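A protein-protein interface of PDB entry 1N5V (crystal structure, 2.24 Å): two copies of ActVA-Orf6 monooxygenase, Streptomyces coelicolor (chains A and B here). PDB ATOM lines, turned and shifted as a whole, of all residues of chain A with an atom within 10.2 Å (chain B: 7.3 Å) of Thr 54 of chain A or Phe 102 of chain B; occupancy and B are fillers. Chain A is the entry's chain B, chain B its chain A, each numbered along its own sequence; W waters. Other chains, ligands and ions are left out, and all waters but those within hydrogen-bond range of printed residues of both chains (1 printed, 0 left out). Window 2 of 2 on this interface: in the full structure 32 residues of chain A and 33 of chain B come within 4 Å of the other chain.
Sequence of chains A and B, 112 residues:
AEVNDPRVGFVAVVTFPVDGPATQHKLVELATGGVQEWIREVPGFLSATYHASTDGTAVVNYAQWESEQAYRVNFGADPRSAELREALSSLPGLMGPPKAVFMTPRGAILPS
Printed residues of chain A that touch a printed residue of chain B: His 51, Ala 52, Ser 53, Thr 54 and Val 60. Of the 13 printed residues of chain B, 4 touch a printed residue of chain A. Hydrophobic or aromatic side chains of chain B that line the printed part of chain A: Val 11, Phe 102 and Met 103.
Water W1 lies within hydrogen-bond range of OG1 of Thr 54 of chain A (2.5 Å), N of Asp 55 of chain A (2.6 Å) and O of Phe 102 of chain B (3.3 Å).
His 51 of chain A touches Val 11 of chain B. Met 103 of chain B touches His 51 of chain A (SD to CG, 3.6 Å). His 51 of chain A touches Thr 104 of chain B (CA to O, 3.2 Å). Ala 52 of chain A touches Met 103 of chain B. Phe 102 of chain B touches Ser 53 of chain A (O to CA, 3.2 Å). Ser 53 of chain A touches Met 103 of chain B (CA to CB, 3.7 Å). CG2 of Thr 54 of chain A touches N of Met 103 of chain B, 3.7 Å away. Val 60 of chain A touches Met 103 of chain B (CG2 to CE, 3.5 Å).
The backbone carbonyl oxygen (O) of Phe 102 of chain B sits at hydrogen-bond distance from the backbone NH (N) of Thr 54 of chain A, at 3.0 Å. N of Thr 104 of chain B lies within hydrogen-bond range of O of Ala 52 of chain A, 2.9 Å away.
No position is printed for both chains. Of the 10 pairs that touch across the chains among the printed residues, none has its exchanged pair printed and touching as well.
The backbone carbonyl oxygen (O) of Met 103 of chain B sits at hydrogen-bond distance from the backbone NH (N) of Val 11 of chain B, 2.8 Å away. The backbone NH (N) of Ser 53 of chain A lies within hydrogen-bond range of the backbone carbonyl oxygen (O) of Ala 58 of chain A (3.0 Å). N of His 51 of chain A sits at hydrogen-bond distance from O of Val 60 of chain A (2.7 Å). OG of Ser 53 of chain A sits at hydrogen-bond distance from N of Thr 57 of chain A. The side-chain carboxylate (OD1) of Asp 55 of chain A is in hydrogen-bond range of the side-chain hydroxyl (OG) of Ser 53 of chain A, at 2.7 Å. The backbone carbonyl oxygen of Ser 53 of chain A sits at hydrogen-bond distance from the side-chain amide nitrogen of Gln 24 of chain A (3.1 Å).
Printed residues of chain A within 4 Å of Phe 102 of chain B: Ser 53 and Thr 54. No residue of chain A comes within 4 Å of Val 101 of chain B. Met 103 of chain B touches just these residues of chain A: His 51 (3.6 Å), Ala 52 (3.3 Å), Ser 53 (3.7 Å), Thr 54 (3.7 Å) and Val 60 (3.5 Å). Of the printed residues of chain B, Val 60 of chain A touches Met 103. Printed residues of chain B within 4 Å of Ala 52 of chain A: Met 103 (3.3 Å) and Thr 104 (2.9 Å). Printed residues of chain B within 4 Å of His 51 of chain A: Val 11 (3.97 Å), Met 103 (3.6 Å) and Thr 104 (3.2 Å). Of the printed residues of chain B, Ser 53 of chain A touches Phe 102 and Met 103. Thr 57 of chain A touches none of the printed residues of chain B. Phe 10 of chain B touches none of the printed residues of chain A. The nearest residue of chain A that does not touch Phe 102 of chain B is Ala 52 of chain A (4.5 Å).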
ATOM      1  N   THR A  15       1.819 -18.024  12.034  1.00  0.00           N
ATOM      2  CA  THR A  15       0.800 -17.261  11.299  1.00  0.00           C
ATOM      3  C   THR A  15       1.418 -16.287  10.316  1.00  0.00           C
ATOM      4  O   THR A  15       2.230 -15.460  10.662  1.00  0.00           O
ATOM      5  CB  THR A  15      -0.095 -16.487  12.287  1.00  0.00           C
ATOM      6  OG1 THR A  15      -0.636 -17.502  13.130  1.00  0.00           O
ATOM      7  CG2 THR A  15      -1.305 -15.763  11.673  1.00  0.00           C
ATOM      8  N   VAL A  18      -1.447 -12.055   5.406  1.00  0.00           N
ATOM      9  CA  VAL A  18      -1.536 -11.895   3.994  1.00  0.00           C
ATOM     10  C   VAL A  18      -2.666 -10.933   3.584  1.00  0.00           C
ATOM     11  O   VAL A  18      -3.649 -10.691   4.288  1.00  0.00           O
ATOM     12  CB  VAL A  18      -1.682 -13.201   3.197  1.00  0.00           C
ATOM     13  CG1 VAL A  18      -0.425 -14.068   3.317  1.00  0.00           C
ATOM     14  CG2 VAL A  18      -2.924 -13.981   3.572  1.00  0.00           C
ATOM     15  N   GLY A  20      -4.861 -11.268   1.140  1.00  0.00           N
ATOM     16  CA  GLY A  20      -6.230 -11.736   0.851  1.00  0.00           C
ATOM     17  C   GLY A  20      -6.173 -13.188   0.429  1.00  0.00           C
ATOM     18  O   GLY A  20      -5.113 -13.779   0.436  1.00  0.00           O
ATOM     19  N   PRO A  21      -7.311 -13.710   0.034  1.00  0.00           N
ATOM     20  CA  PRO A  21      -7.439 -15.072  -0.380  1.00  0.00           C
ATOM     21  C   PRO A  21      -6.518 -15.502  -1.472  1.00  0.00           C
ATOM     22  O   PRO A  21      -6.148 -16.680  -1.474  1.00  0.00           O
ATOM     23  CB  PRO A  21      -8.897 -15.170  -0.856  1.00  0.00           C
ATOM     24  CG  PRO A  21      -9.640 -14.071  -0.164  1.00  0.00           C
ATOM     25  CD  PRO A  21      -8.626 -12.969   0.026  1.00  0.00           C
ATOM     26  N   GLN A  24      -3.296 -16.220   0.094  1.00  0.00           N
ATOM     27  CA  GLN A  24      -3.443 -17.354   0.976  1.00  0.00           C
ATOM     28  C   GLN A  24      -3.158 -18.646   0.188  1.00  0.00           C
ATOM     29  O   GLN A  24      -2.387 -19.516   0.518  1.00  0.00           O
ATOM     30  CB  GLN A  24      -4.867 -17.482   1.532  1.00  0.00           C
ATOM     31  CG  GLN A  24      -5.290 -16.453   2.559  1.00  0.00           C
ATOM     32  CD  GLN A  24      -6.713 -16.706   3.018  1.00  0.00           C
ATOM     33  OE1 GLN A  24      -7.623 -16.985   2.198  1.00  0.00           O
ATOM     34  NE2 GLN A  24      -6.900 -16.620   4.339  1.00  0.00           N
ATOM     35  N   HIS A  51      -3.584 -23.791   7.062  1.00  0.00           N
ATOM     36  CA  HIS A  51      -4.989 -23.357   7.038  1.00  0.00           C
ATOM     37  C   HIS A  51      -5.163 -21.931   6.522  1.00  0.00           C
ATOM     38  O   HIS A  51      -4.368 -21.062   6.777  1.00  0.00           O
ATOM     39  CB  HIS A  51      -5.608 -23.326   8.439  1.00  0.00           C
ATOM     40  CG  HIS A  51      -5.272 -24.473   9.345  1.00  0.00           C
ATOM     41  ND1 HIS A  51      -3.984 -24.677   9.861  1.00  0.00           N
ATOM     42  CD2 HIS A  51      -6.060 -25.471   9.821  1.00  0.00           C
ATOM     43  CE1 HIS A  51      -4.011 -25.748  10.613  1.00  0.00           C
ATOM     44  NE2 HIS A  51      -5.256 -26.221  10.626  1.00  0.00           N
ATOM     45  N   ALA A  52      -6.346 -21.665   5.981  1.00  0.00           N
ATOM     46  CA  ALA A  52      -6.754 -20.354   5.505  1.00  0.00           C
ATOM     47  C   ALA A  52      -7.744 -19.772   6.510  1.00  0.00           C
ATOM     48  O   ALA A  52      -8.764 -20.416   6.775  1.00  0.00           O
ATOM     49  CB  ALA A  52      -7.474 -20.443   4.146  1.00  0.00           C
ATOM     50  N   SER A  53      -7.350 -18.654   7.145  1.00  0.00           N
ATOM     51  CA  SER A  53      -8.348 -18.096   8.051  1.00  0.00           C
ATOM     52  C   SER A  53      -9.553 -17.745   7.154  1.00  0.00           C
ATOM     53  O   SER A  53      -9.442 -17.323   6.000  1.00  0.00           O
ATOM     54  CB  SER A  53      -7.916 -16.826   8.757  1.00  0.00           C
ATOM     55  OG  SER A  53      -7.783 -15.742   7.857  1.00  0.00           O
ATOM     56  N   THR A  54     -10.706 -17.818   7.790  1.00  0.00           N
ATOM     57  CA  THR A  54     -11.982 -17.559   7.144  1.00  0.00           C
ATOM     58  C   THR A  54     -12.041 -16.135   6.629  1.00  0.00           C
ATOM     59  O   THR A  54     -12.563 -15.925   5.556  1.00  0.00           O
ATOM     60  CB  THR A  54     -13.173 -17.879   8.058  1.00  0.00           C
ATOM     61  OG1 THR A  54     -13.026 -17.099   9.253  1.00  0.00           O
ATOM     62  CG2 THR A  54     -13.196 -19.331   8.496  1.00  0.00           C
ATOM     63  N   ASP A  55     -11.403 -15.154   7.244  1.00  0.00           N
ATOM     64  CA  ASP A  55     -11.497 -13.785   6.751  1.00  0.00           C
ATOM     65  C   ASP A  55     -10.513 -13.480   5.655  1.00  0.00           C
ATOM     66  O   ASP A  55     -10.235 -12.314   5.356  1.00  0.00           O
ATOM     67  CB  ASP A  55     -11.385 -12.891   7.980  1.00  0.00           C
ATOM     68  CG  ASP A  55      -9.981 -12.818   8.555  1.00  0.00           C
ATOM     69  OD1 ASP A  55      -9.051 -13.413   7.984  1.00  0.00           O
ATOM     70  OD2 ASP A  55      -9.881 -12.131   9.585  1.00  0.00           O
ATOM     71  N   GLY A  56      -9.860 -14.487   5.064  1.00  0.00           N
ATOM     72  CA  GLY A  56      -8.875 -14.270   4.024  1.00  0.00           C
ATOM     73  C   GLY A  56      -7.670 -13.471   4.486  1.00  0.00           C
ATOM     74  O   GLY A  56      -6.849 -13.262   3.571  1.00  0.00           O
ATOM     75  N   THR A  57      -7.405 -13.139   5.758  1.00  0.00           N
ATOM     76  CA  THR A  57      -6.231 -12.349   6.068  1.00  0.00           C
ATOM     77  C   THR A  57      -5.031 -13.145   6.557  1.00  0.00           C
ATOM     78  O   THR A  57      -4.037 -12.504   6.939  1.00  0.00           O
ATOM     79  CB  THR A  57      -6.492 -11.261   7.149  1.00  0.00           C
ATOM     80  OG1 THR A  57      -6.690 -11.882   8.413  1.00  0.00           O
ATOM     81  CG2 THR A  57      -7.723 -10.431   6.829  1.00  0.00           C
ATOM     82  N   ALA A  58      -5.078 -14.472   6.576  1.00  0.00           N
ATOM     83  CA  ALA A  58      -3.933 -15.183   7.182  1.00  0.00           C
ATOM     84  C   ALA A  58      -3.827 -16.633   6.786  1.00  0.00           C
ATOM     85  O   ALA A  58      -4.808 -17.290   6.513  1.00  0.00           O
ATOM     86  CB  ALA A  58      -4.065 -15.014   8.691  1.00  0.00           C
ATOM     87  N   VAL A  59      -2.602 -17.177   6.870  1.00  0.00           N
ATOM     88  CA  VAL A  59      -2.354 -18.609   6.662  1.00  0.00           C
ATOM     89  C   VAL A  59      -1.719 -19.117   7.957  1.00  0.00           C
ATOM     90  O   VAL A  59      -0.800 -18.483   8.479  1.00  0.00           O
ATOM     91  CB  VAL A  59      -1.341 -18.931   5.560  1.00  0.00           C
ATOM     92  CG1 VAL A  59      -0.999 -20.426   5.512  1.00  0.00           C
ATOM     93  CG2 VAL A  59      -1.955 -18.450   4.240  1.00  0.00           C
ATOM     94  N   VAL A  60      -2.280 -20.166   8.522  1.00  0.00           N
ATOM     95  CA  VAL A  60      -1.738 -20.633   9.806  1.00  0.00           C
ATOM     96  C   VAL A  60      -1.275 -22.087   9.622  1.00  0.00           C
ATOM     97  O   VAL A  60      -1.929 -22.941   9.026  1.00  0.00           O
ATOM     98  CB  VAL A  60      -2.782 -20.548  10.930  1.00  0.00           C
ATOM     99  CG1 VAL A  60      -2.215 -21.104  12.216  1.00  0.00           C
ATOM    100  CG2 VAL A  60      -3.390 -19.148  11.087  1.00  0.00           C
ATOM    101  N   GLY B   9     -13.509 -29.927   8.755  1.00  0.00           N
ATOM    102  CA  GLY B   9     -13.946 -28.818   7.893  1.00  0.00           C
ATOM    103  C   GLY B   9     -13.731 -27.454   8.535  1.00  0.00           C
ATOM    104  O   GLY B   9     -13.869 -26.469   7.845  1.00  0.00           O
ATOM    105  N   PHE B  10     -13.421 -27.386   9.825  1.00  0.00           N
ATOM    106  CA  PHE B  10     -13.349 -26.105  10.477  1.00  0.00           C
ATOM    107  C   PHE B  10     -12.524 -26.237  11.741  1.00  0.00           C
ATOM    108  O   PHE B  10     -12.676 -27.180  12.488  1.00  0.00           O
ATOM    109  CB  PHE B  10     -14.767 -25.610  10.774  1.00  0.00           C
ATOM    110  CG  PHE B  10     -14.923 -24.234  11.354  1.00  0.00           C
ATOM    111  CD1 PHE B  10     -14.965 -23.119  10.534  1.00  0.00           C
ATOM    112  CD2 PHE B  10     -15.046 -24.054  12.721  1.00  0.00           C
ATOM    113  CE1 PHE B  10     -15.088 -21.846  11.063  1.00  0.00           C
ATOM    114  CE2 PHE B  10     -15.182 -22.781  13.245  1.00  0.00           C
ATOM    115  CZ  PHE B  10     -15.255 -21.670  12.426  1.00  0.00           C
ATOM    116  N   VAL B  11     -11.683 -25.247  11.960  1.00  0.00           N
ATOM    117  CA  VAL B  11     -10.755 -25.158  13.053  1.00  0.00           C
ATOM    118  C   VAL B  11     -10.896 -23.817  13.736  1.00  0.00           C
ATOM    119  O   VAL B  11     -10.917 -22.725  13.170  1.00  0.00           O
ATOM    120  CB  VAL B  11      -9.314 -25.377  12.519  1.00  0.00           C
ATOM    121  CG1 VAL B  11      -8.231 -25.104  13.575  1.00  0.00           C
ATOM    122  CG2 VAL B  11      -9.121 -26.794  11.980  1.00  0.00           C
ATOM    123  N   ALA B  12     -10.889 -23.865  15.051  1.00  0.00           N
ATOM    124  CA  ALA B  12     -10.864 -22.711  15.951  1.00  0.00           C
ATOM    125  C   ALA B  12      -9.573 -22.845  16.773  1.00  0.00           C
ATOM    126  O   ALA B  12      -9.253 -23.845  17.421  1.00  0.00           O
ATOM    127  CB  ALA B  12     -12.098 -22.709  16.855  1.00  0.00           C
ATOM    128  N   VAL B  13      -8.750 -21.826  16.735  1.00  0.00           N
ATOM    129  CA  VAL B  13      -7.507 -21.750  17.495  1.00  0.00           C
ATOM    130  C   VAL B  13      -7.771 -20.663  18.527  1.00  0.00           C
ATOM    131  O   VAL B  13      -7.931 -19.504  18.177  1.00  0.00           O
ATOM    132  CB  VAL B  13      -6.337 -21.365  16.591  1.00  0.00           C
ATOM    133  CG1 VAL B  13      -5.096 -21.172  17.443  1.00  0.00           C
ATOM    134  CG2 VAL B  13      -6.143 -22.418  15.511  1.00  0.00           C
ATOM    135  N   VAL B  14      -7.857 -21.039  19.774  1.00  0.00           N
ATOM    136  CA  VAL B  14      -8.235 -20.183  20.871  1.00  0.00           C
ATOM    137  C   VAL B  14      -7.044 -20.070  21.819  1.00  0.00           C
ATOM    138  O   VAL B  14      -6.693 -21.034  22.478  1.00  0.00           O
ATOM    139  CB  VAL B  14      -9.447 -20.742  21.652  1.00  0.00           C
ATOM    140  CG1 VAL B  14      -9.929 -19.758  22.704  1.00  0.00           C
ATOM    141  CG2 VAL B  14     -10.636 -21.072  20.741  1.00  0.00           C
ATOM    142  N   GLU B  68     -18.372 -25.570   9.884  1.00  0.00           N
ATOM    143  CA  GLU B  68     -18.761 -24.362  10.618  1.00  0.00           C
ATOM    144  C   GLU B  68     -20.173 -24.452  11.144  1.00  0.00           C
ATOM    145  O   GLU B  68     -20.572 -23.955  12.241  1.00  0.00           O
ATOM    146  CB  GLU B  68     -18.617 -23.154   9.641  1.00  0.00           C
ATOM    147  CG  GLU B  68     -18.811 -21.846  10.365  1.00  0.00           C
ATOM    148  CD  GLU B  68     -18.828 -20.574   9.525  1.00  0.00           C
ATOM    149  OE1 GLU B  68     -18.233 -20.442   8.434  1.00  0.00           O
ATOM    150  OE2 GLU B  68     -19.491 -19.621   9.984  1.00  0.00           O
ATOM    151  N   TYR B  71     -20.225 -26.432  14.210  1.00  0.00           N
ATOM    152  CA  TYR B  71     -19.693 -25.584  15.271  1.00  0.00           C
ATOM    153  C   TYR B  71     -20.708 -24.544  15.740  1.00  0.00           C
ATOM    154  O   TYR B  71     -20.842 -24.224  16.945  1.00  0.00           O
ATOM    155  CB  TYR B  71     -18.448 -24.846  14.754  1.00  0.00           C
ATOM    156  CG  TYR B  71     -17.896 -23.791  15.705  1.00  0.00           C
ATOM    157  CD1 TYR B  71     -17.045 -24.234  16.717  1.00  0.00           C
ATOM    158  CD2 TYR B  71     -18.208 -22.432  15.638  1.00  0.00           C
ATOM    159  CE1 TYR B  71     -16.508 -23.378  17.645  1.00  0.00           C
ATOM    160  CE2 TYR B  71     -17.657 -21.532  16.556  1.00  0.00           C
ATOM    161  CZ  TYR B  71     -16.813 -22.023  17.531  1.00  0.00           C
ATOM    162  OH  TYR B  71     -16.207 -21.240  18.498  1.00  0.00           O
ATOM    163  N   ALA B 100      -9.836 -15.759  19.515  1.00  0.00           N
ATOM    164  CA  ALA B 100     -10.124 -16.872  18.635  1.00  0.00           C
ATOM    165  C   ALA B 100      -9.866 -16.560  17.171  1.00  0.00           C
ATOM    166  O   ALA B 100     -10.061 -15.416  16.737  1.00  0.00           O
ATOM    167  CB  ALA B 100     -11.567 -17.297  18.790  1.00  0.00           C
ATOM    168  N   VAL B 101      -9.310 -17.532  16.477  1.00  0.00           N
ATOM    169  CA  VAL B 101      -9.042 -17.394  15.052  1.00  0.00           C
ATOM    170  C   VAL B 101      -9.787 -18.528  14.357  1.00  0.00           C
ATOM    171  O   VAL B 101      -9.734 -19.670  14.816  1.00  0.00           O
ATOM    172  CB  VAL B 101      -7.545 -17.443  14.695  1.00  0.00           C
ATOM    173  CG1 VAL B 101      -7.309 -17.176  13.201  1.00  0.00           C
ATOM    174  CG2 VAL B 101      -6.697 -16.424  15.460  1.00  0.00           C
ATOM    175  N   PHE B 102     -10.637 -18.248  13.389  1.00  0.00           N
ATOM    176  CA  PHE B 102     -11.401 -19.280  12.683  1.00  0.00           C
ATOM    177  C   PHE B 102     -10.701 -19.498  11.345  1.00  0.00           C
ATOM    178  O   PHE B 102     -10.190 -18.606  10.679  1.00  0.00           O
ATOM    179  CB  PHE B 102     -12.883 -18.977  12.602  1.00  0.00           C
ATOM    180  CG  PHE B 102     -13.515 -18.676  13.933  1.00  0.00           C
ATOM    181  CD1 PHE B 102     -13.759 -19.676  14.856  1.00  0.00           C
ATOM    182  CD2 PHE B 102     -13.862 -17.396  14.290  1.00  0.00           C
ATOM    183  CE1 PHE B 102     -14.300 -19.396  16.102  1.00  0.00           C
ATOM    184  CE2 PHE B 102     -14.434 -17.069  15.506  1.00  0.00           C
ATOM    185  CZ  PHE B 102     -14.656 -18.082  16.427  1.00  0.00           C
ATOM    186  N   MET B 103     -10.710 -20.747  10.898  1.00  0.00           N
ATOM    187  CA  MET B 103     -10.004 -21.160   9.740  1.00  0.00           C
ATOM    188  C   MET B 103     -10.368 -22.534   9.249  1.00  0.00           C
ATOM    189  O   MET B 103     -10.877 -23.454   9.904  1.00  0.00           O
ATOM    190  CB  MET B 103      -8.489 -21.096  10.183  1.00  0.00           C
ATOM    191  CG  MET B 103      -8.079 -22.141  11.170  1.00  0.00           C
ATOM    192  SD  MET B 103      -6.364 -22.058  11.764  1.00  0.00           S
ATOM    193  CE  MET B 103      -6.327 -20.458  12.520  1.00  0.00           C
ATOM    194  N   THR B 104      -9.912 -22.742   8.008  1.00  0.00           N
ATOM    195  CA  THR B 104     -10.153 -24.036   7.333  1.00  0.00           C
ATOM    196  C   THR B 104      -8.857 -24.668   6.940  1.00  0.00           C
ATOM    197  O   THR B 104      -8.005 -24.006   6.308  1.00  0.00           O
ATOM    198  CB  THR B 104     -11.032 -23.583   6.128  1.00  0.00           C
ATOM    199  OG1 THR B 104     -12.390 -23.509   6.640  1.00  0.00           O
ATOM    200  CG2 THR B 104     -10.973 -24.446   4.928  1.00  0.00           C
HETATM  201  O   HOH W   1     -11.074 -15.594   9.816  1.00  0.00           O
